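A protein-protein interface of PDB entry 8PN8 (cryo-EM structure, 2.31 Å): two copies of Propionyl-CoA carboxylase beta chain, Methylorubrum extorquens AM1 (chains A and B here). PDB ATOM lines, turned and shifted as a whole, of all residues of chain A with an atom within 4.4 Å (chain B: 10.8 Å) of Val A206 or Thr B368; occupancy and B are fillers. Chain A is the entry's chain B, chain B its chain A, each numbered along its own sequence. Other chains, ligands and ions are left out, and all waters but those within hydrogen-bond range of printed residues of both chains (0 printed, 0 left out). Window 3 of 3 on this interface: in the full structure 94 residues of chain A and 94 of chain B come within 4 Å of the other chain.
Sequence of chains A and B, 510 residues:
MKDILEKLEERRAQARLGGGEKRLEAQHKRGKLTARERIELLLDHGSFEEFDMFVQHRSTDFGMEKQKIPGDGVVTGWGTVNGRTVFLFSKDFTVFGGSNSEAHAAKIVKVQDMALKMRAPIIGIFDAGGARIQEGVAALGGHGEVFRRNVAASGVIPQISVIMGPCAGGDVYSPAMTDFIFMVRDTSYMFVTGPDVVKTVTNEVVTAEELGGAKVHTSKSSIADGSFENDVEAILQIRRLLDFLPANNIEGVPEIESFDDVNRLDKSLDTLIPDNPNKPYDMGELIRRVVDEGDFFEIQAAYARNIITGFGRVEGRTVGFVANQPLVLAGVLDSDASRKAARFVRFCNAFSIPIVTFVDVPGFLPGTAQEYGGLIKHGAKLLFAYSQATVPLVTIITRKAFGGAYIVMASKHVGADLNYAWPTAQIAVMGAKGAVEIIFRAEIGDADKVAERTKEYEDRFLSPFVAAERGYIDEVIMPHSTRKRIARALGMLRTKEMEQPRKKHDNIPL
No position is printed for both chains. Of the 7 pairs that touch across the chains among the printed residues, none has its exchanged pair printed and touching as well.
Of the 15 printed residues of chain B, 4 touch a printed residue of chain A. Of the 8 printed residues of chain A, 5 touch a printed residue of chain B. Hydrophobic or aromatic side chains of chain A within 4 Å of the printed part of chain B: Val A198, Val A206 and Leu A211. Among the printed residues, 7 pairs touch across the chains. Among the printed residues, no Asp or Glu carboxylate lies within 4 Å of a Lys or Arg side-chain nitrogen of the other chain.
The side-chain hydroxyl (OG1) of Thr B368 lies within hydrogen-bond range of the side-chain carboxylate (OE2) of Glu A204, 3.2 Å away. The side-chain hydroxyl of Tyr B372 sits at hydrogen-bond distance from the backbone carbonyl oxygen of Glu A210 (2.8 Å).
The backbone NH of Glu A210 lies within hydrogen-bond range of the side-chain hydroxyl of Thr A207.
Among the printed residues, merely in contact across the chains: Leu A211 with Tyr B372 (3.6 Å), Val A198 with Gly B367 (3.6 Å), Val A206 with Thr B368 (3.7 Å), Leu A211 with Glu B371 (3.7 Å) and Leu A211 with Thr B368 (3.7 Å).
Of chain B, only Thr B368 comes within 4 Å of Val A206. Thr B368 touches just these residues of chain A: Glu A204, Val A206 and Leu A211. Glu A204 touches one residue of chain B. Of the printed residues of chain B, Val A198 touches Gly B367. Printed residues of chain A within 4 Å of Glu B371: Leu A211. Printed residues of chain A within 4 Å of Gly B367: Val A198 (3.6 Å). Printed residues of chain A within 4 Å of Tyr B372: Glu A210 (2.8 Å) and Leu A211 (3.6 Å). Gly B373 touches none of the printed residues of chain A.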
ATOM      1  N   PRO A 195     -18.588   3.162  11.827  1.00  0.00           N
ATOM      2  CA  PRO A 195     -19.738   2.541  12.505  1.00  0.00           C
ATOM      3  C   PRO A 195     -19.736   2.711  14.015  1.00  0.00           C
ATOM      4  O   PRO A 195     -20.815   2.785  14.615  1.00  0.00           O
ATOM      5  CB  PRO A 195     -19.617   1.062  12.107  1.00  0.00           C
ATOM      6  CG  PRO A 195     -18.819   1.071  10.851  1.00  0.00           C
ATOM      7  CD  PRO A 195     -17.847   2.198  10.999  1.00  0.00           C
ATOM      8  N   VAL A 198     -21.101   6.095  14.839  1.00  0.00           N
ATOM      9  CA  VAL A 198     -22.520   6.074  14.497  1.00  0.00           C
ATOM     10  C   VAL A 198     -23.318   5.388  15.596  1.00  0.00           C
ATOM     11  O   VAL A 198     -24.383   5.867  16.003  1.00  0.00           O
ATOM     12  CB  VAL A 198     -22.731   5.392  13.132  1.00  0.00           C
ATOM     13  CG1 VAL A 198     -24.206   5.129  12.889  1.00  0.00           C
ATOM     14  CG2 VAL A 198     -22.157   6.249  12.019  1.00  0.00           C
ATOM     15  N   GLU A 204     -27.459   3.596  16.300  1.00  0.00           N
ATOM     16  CA  GLU A 204     -27.785   2.751  15.160  1.00  0.00           C
ATOM     17  C   GLU A 204     -26.663   1.748  14.945  1.00  0.00           C
ATOM     18  O   GLU A 204     -25.484   2.114  14.980  1.00  0.00           O
ATOM     19  CB  GLU A 204     -28.001   3.590  13.899  1.00  0.00           C
ATOM     20  CG  GLU A 204     -28.427   2.785  12.685  1.00  0.00           C
ATOM     21  CD  GLU A 204     -28.703   3.656  11.477  1.00  0.00           C
ATOM     22  OE1 GLU A 204     -28.500   4.885  11.570  1.00  0.00           O
ATOM     23  OE2 GLU A 204     -29.124   3.112  10.436  1.00  0.00           O
ATOM     24  N   VAL A 205     -27.031   0.491  14.725  1.00  0.00           N
ATOM     25  CA  VAL A 205     -26.071  -0.592  14.552  1.00  0.00           C
ATOM     26  C   VAL A 205     -25.976  -0.900  13.065  1.00  0.00           C
ATOM     27  O   VAL A 205     -26.921  -1.424  12.467  1.00  0.00           O
ATOM     28  CB  VAL A 205     -26.472  -1.837  15.353  1.00  0.00           C
ATOM     29  CG1 VAL A 205     -25.467  -2.955  15.131  1.00  0.00           C
ATOM     30  CG2 VAL A 205     -26.585  -1.501  16.828  1.00  0.00           C
ATOM     31  N   VAL A 206     -24.832  -0.574  12.462  1.00  0.00           N
ATOM     32  CA  VAL A 206     -24.559  -0.883  11.066  1.00  0.00           C
ATOM     33  C   VAL A 206     -23.144  -1.429  10.958  1.00  0.00           C
ATOM     34  O   VAL A 206     -22.283  -1.161  11.798  1.00  0.00           O
ATOM     35  CB  VAL A 206     -24.725   0.344  10.140  1.00  0.00           C
ATOM     36  CG1 VAL A 206     -26.176   0.785  10.087  1.00  0.00           C
ATOM     37  CG2 VAL A 206     -23.832   1.483  10.603  1.00  0.00           C
ATOM     38  N   THR A 207     -22.912  -2.206   9.908  1.00  0.00           N
ATOM     39  CA  THR A 207     -21.572  -2.673   9.597  1.00  0.00           C
ATOM     40  C   THR A 207     -20.904  -1.715   8.616  1.00  0.00           C
ATOM     41  O   THR A 207     -21.511  -0.761   8.129  1.00  0.00           O
ATOM     42  CB  THR A 207     -21.609  -4.090   9.022  1.00  0.00           C
ATOM     43  OG1 THR A 207     -22.233  -4.070   7.733  1.00  0.00           O
ATOM     44  CG2 THR A 207     -22.390  -5.014   9.937  1.00  0.00           C
ATOM     45  N   GLU A 210     -22.689  -2.144   5.240  1.00  0.00           N
ATOM     46  CA  GLU A 210     -23.988  -1.480   5.220  1.00  0.00           C
ATOM     47  C   GLU A 210     -23.835   0.034   5.176  1.00  0.00           C
ATOM     48  O   GLU A 210     -24.582   0.719   4.468  1.00  0.00           O
ATOM     49  CB  GLU A 210     -24.809  -1.897   6.439  1.00  0.00           C
ATOM     50  CG  GLU A 210     -25.130  -3.379   6.503  1.00  0.00           C
ATOM     51  CD  GLU A 210     -25.860  -3.761   7.776  1.00  0.00           C
ATOM     52  OE1 GLU A 210     -26.288  -2.849   8.514  1.00  0.00           O
ATOM     53  OE2 GLU A 210     -26.000  -4.972   8.042  1.00  0.00           O
ATOM     54  N   LEU A 211     -22.879   0.574   5.932  1.00  0.00           N
ATOM     55  CA  LEU A 211     -22.735   2.022   6.021  1.00  0.00           C
ATOM     56  C   LEU A 211     -22.156   2.609   4.739  1.00  0.00           C
ATOM     57  O   LEU A 211     -22.663   3.610   4.221  1.00  0.00           O
ATOM     58  CB  LEU A 211     -21.861   2.382   7.222  1.00  0.00           C
ATOM     59  CG  LEU A 211     -21.678   3.869   7.515  1.00  0.00           C
ATOM     60  CD1 LEU A 211     -23.020   4.538   7.750  1.00  0.00           C
ATOM     61  CD2 LEU A 211     -20.769   4.057   8.713  1.00  0.00           C
ATOM     62  N   SER B 335     -24.390  17.785   5.020  1.00  0.00           N
ATOM     63  CA  SER B 335     -24.504  18.049   3.589  1.00  0.00           C
ATOM     64  C   SER B 335     -25.103  19.424   3.318  1.00  0.00           C
ATOM     65  O   SER B 335     -24.610  20.164   2.458  1.00  0.00           O
ATOM     66  CB  SER B 335     -25.344  16.959   2.926  1.00  0.00           C
ATOM     67  OG  SER B 335     -24.763  15.683   3.115  1.00  0.00           O
ATOM     68  N   PHE B 364     -18.097  16.085  11.640  1.00  0.00           N
ATOM     69  CA  PHE B 364     -19.201  15.940  10.706  1.00  0.00           C
ATOM     70  C   PHE B 364     -20.346  15.177  11.357  1.00  0.00           C
ATOM     71  O   PHE B 364     -20.163  14.446  12.335  1.00  0.00           O
ATOM     72  CB  PHE B 364     -18.750  15.226   9.429  1.00  0.00           C
ATOM     73  CG  PHE B 364     -17.718  15.982   8.647  1.00  0.00           C
ATOM     74  CD1 PHE B 364     -18.096  16.919   7.704  1.00  0.00           C
ATOM     75  CD2 PHE B 364     -16.369  15.763   8.862  1.00  0.00           C
ATOM     76  CE1 PHE B 364     -17.150  17.622   6.988  1.00  0.00           C
ATOM     77  CE2 PHE B 364     -15.418  16.461   8.149  1.00  0.00           C
ATOM     78  CZ  PHE B 364     -15.809  17.392   7.210  1.00  0.00           C
ATOM     79  N   LEU B 365     -21.534  15.359  10.803  1.00  0.00           N
ATOM     80  CA  LEU B 365     -22.719  14.685  11.316  1.00  0.00           C
ATOM     81  C   LEU B 365     -22.669  13.209  10.947  1.00  0.00           C
ATOM     82  O   LEU B 365     -22.539  12.882   9.760  1.00  0.00           O
ATOM     83  CB  LEU B 365     -23.978  15.335  10.753  1.00  0.00           C
ATOM     84  CG  LEU B 365     -25.320  14.850  11.300  1.00  0.00           C
ATOM     85  CD1 LEU B 365     -25.446  15.177  12.775  1.00  0.00           C
ATOM     86  CD2 LEU B 365     -26.463  15.461  10.515  1.00  0.00           C
ATOM     87  N   PRO B 366     -22.764  12.294  11.905  1.00  0.00           N
ATOM     88  CA  PRO B 366     -22.703  10.868  11.591  1.00  0.00           C
ATOM     89  C   PRO B 366     -24.089  10.276  11.350  1.00  0.00           C
ATOM     90  O   PRO B 366     -25.119  10.893  11.623  1.00  0.00           O
ATOM     91  CB  PRO B 366     -22.061  10.268  12.850  1.00  0.00           C
ATOM     92  CG  PRO B 366     -22.316  11.280  13.954  1.00  0.00           C
ATOM     93  CD  PRO B 366     -22.905  12.526  13.350  1.00  0.00           C
ATOM     94  N   GLY B 367     -24.088   9.055  10.823  1.00  0.00           N
ATOM     95  CA  GLY B 367     -25.322   8.337  10.579  1.00  0.00           C
ATOM     96  C   GLY B 367     -25.462   7.845   9.154  1.00  0.00           C
ATOM     97  O   GLY B 367     -24.742   8.298   8.261  1.00  0.00           O
ATOM     98  N   THR B 368     -26.391   6.914   8.930  1.00  0.00           N
ATOM     99  CA  THR B 368     -26.608   6.402   7.583  1.00  0.00           C
ATOM    100  C   THR B 368     -27.311   7.421   6.697  1.00  0.00           C
ATOM    101  O   THR B 368     -27.158   7.380   5.473  1.00  0.00           O
ATOM    102  CB  THR B 368     -27.415   5.105   7.628  1.00  0.00           C
ATOM    103  OG1 THR B 368     -28.680   5.348   8.256  1.00  0.00           O
ATOM    104  CG2 THR B 368     -26.666   4.043   8.406  1.00  0.00           C
ATOM    105  N   ALA B 369     -28.086   8.332   7.289  1.00  0.00           N
ATOM    106  CA  ALA B 369     -28.786   9.334   6.491  1.00  0.00           C
ATOM    107  C   ALA B 369     -27.805  10.245   5.765  1.00  0.00           C
ATOM    108  O   ALA B 369     -28.019  10.596   4.599  1.00  0.00           O
ATOM    109  CB  ALA B 369     -29.721  10.153   7.379  1.00  0.00           C
ATOM    110  N   GLN B 370     -26.727  10.646   6.440  1.00  0.00           N
ATOM    111  CA  GLN B 370     -25.731  11.498   5.801  1.00  0.00           C
ATOM    112  C   GLN B 370     -24.938  10.736   4.747  1.00  0.00           C
ATOM    113  O   GLN B 370     -24.684  11.259   3.656  1.00  0.00           O
ATOM    114  CB  GLN B 370     -24.796  12.092   6.853  1.00  0.00           C
ATOM    115  CG  GLN B 370     -25.449  13.148   7.719  1.00  0.00           C
ATOM    116  CD  GLN B 370     -25.900  14.350   6.918  1.00  0.00           C
ATOM    117  OE1 GLN B 370     -25.186  14.826   6.039  1.00  0.00           O
ATOM    118  NE2 GLN B 370     -27.096  14.841   7.211  1.00  0.00           N
ATOM    119  N   GLU B 371     -24.535   9.502   5.053  1.00  0.00           N
ATOM    120  CA  GLU B 371     -23.725   8.736   4.112  1.00  0.00           C
ATOM    121  C   GLU B 371     -24.514   8.374   2.860  1.00  0.00           C
ATOM    122  O   GLU B 371     -23.983   8.436   1.746  1.00  0.00           O
ATOM    123  CB  GLU B 371     -23.183   7.479   4.789  1.00  0.00           C
ATOM    124  CG  GLU B 371     -22.358   7.757   6.033  1.00  0.00           C
ATOM    125  CD  GLU B 371     -21.087   8.535   5.740  1.00  0.00           C
ATOM    126  OE1 GLU B 371     -20.575   8.444   4.605  1.00  0.00           O
ATOM    127  OE2 GLU B 371     -20.599   9.237   6.649  1.00  0.00           O
ATOM    128  N   TYR B 372     -25.783   7.993   3.019  1.00  0.00           N
ATOM    129  CA  TYR B 372     -26.608   7.654   1.867  1.00  0.00           C
ATOM    130  C   TYR B 372     -26.979   8.881   1.051  1.00  0.00           C
ATOM    131  O   TYR B 372     -27.282   8.752  -0.138  1.00  0.00           O
ATOM    132  CB  TYR B 372     -27.879   6.928   2.310  1.00  0.00           C
ATOM    133  CG  TYR B 372     -27.646   5.597   2.993  1.00  0.00           C
ATOM    134  CD1 TYR B 372     -26.402   4.982   2.964  1.00  0.00           C
ATOM    135  CD2 TYR B 372     -28.676   4.953   3.660  1.00  0.00           C
ATOM    136  CE1 TYR B 372     -26.191   3.770   3.586  1.00  0.00           C
ATOM    137  CE2 TYR B 372     -28.474   3.739   4.282  1.00  0.00           C
ATOM    138  CZ  TYR B 372     -27.230   3.153   4.243  1.00  0.00           C
ATOM    139  OH  TYR B 372     -27.024   1.944   4.863  1.00  0.00           O
ATOM    140  N   GLY B 373     -26.970  10.060   1.662  1.00  0.00           N
ATOM    141  CA  GLY B 373     -27.237  11.293   0.958  1.00  0.00           C
ATOM    142  C   GLY B 373     -26.054  11.889   0.240  1.00  0.00           C
ATOM    143  O   GLY B 373     -26.181  12.957  -0.363  1.00  0.00           O
ATOM    144  N   GLY B 374     -24.902  11.231   0.287  1.00  0.00           N
ATOM    145  CA  GLY B 374     -23.718  11.748  -0.370  1.00  0.00           C
ATOM    146  C   GLY B 374     -22.945  12.759   0.444  1.00  0.00           C
ATOM    147  O   GLY B 374     -22.521  13.787  -0.097  1.00  0.00           O
ATOM    148  N   LEU B 375     -22.746  12.495   1.738  1.00  0.00           N
ATOM    149  CA  LEU B 375     -22.007  13.430   2.579  1.00  0.00           C
ATOM    150  C   LEU B 375     -20.573  13.605   2.104  1.00  0.00           C
ATOM    151  O   LEU B 375     -19.981  14.667   2.308  1.00  0.00           O
ATOM    152  CB  LEU B 375     -22.026  12.964   4.036  1.00  0.00           C
ATOM    153  CG  LEU B 375     -21.215  13.793   5.036  1.00  0.00           C
ATOM    154  CD1 LEU B 375     -21.694  15.232   5.066  1.00  0.00           C
ATOM    155  CD2 LEU B 375     -21.269  13.179   6.424  1.00  0.00           C
ATOM    156  N   ILE B 376     -19.999  12.586   1.465  1.00  0.00           N
ATOM    157  CA  ILE B 376     -18.614  12.686   1.011  1.00  0.00           C
ATOM    158  C   ILE B 376     -18.469  13.811  -0.009  1.00  0.00           C
ATOM    159  O   ILE B 376     -17.663  14.732   0.166  1.00  0.00           O
ATOM    160  CB  ILE B 376     -18.141  11.336   0.445  1.00  0.00           C
ATOM    161  CG1 ILE B 376     -18.321  10.233   1.489  1.00  0.00           C
ATOM    162  CG2 ILE B 376     -16.695  11.412   0.015  1.00  0.00           C
ATOM    163  CD1 ILE B 376     -17.889   8.865   1.017  1.00  0.00           C
ATOM    164  N   HIS B 378     -20.784  16.169  -0.872  1.00  0.00           N
ATOM    165  CA  HIS B 378     -21.314  17.436  -0.378  1.00  0.00           C
ATOM    166  C   HIS B 378     -20.318  18.128   0.545  1.00  0.00           C
ATOM    167  O   HIS B 378     -20.139  19.348   0.471  1.00  0.00           O
ATOM    168  CB  HIS B 378     -22.647  17.202   0.331  1.00  0.00           C
ATOM    169  CG  HIS B 378     -23.709  16.639  -0.560  1.00  0.00           C
ATOM    170  ND1 HIS B 378     -23.701  16.816  -1.927  1.00  0.00           N
ATOM    171  CD2 HIS B 378     -24.804  15.893  -0.284  1.00  0.00           C
ATOM    172  CE1 HIS B 378     -24.749  16.208  -2.453  1.00  0.00           C
ATOM    173  NE2 HIS B 378     -25.434  15.640  -1.478  1.00  0.00           N
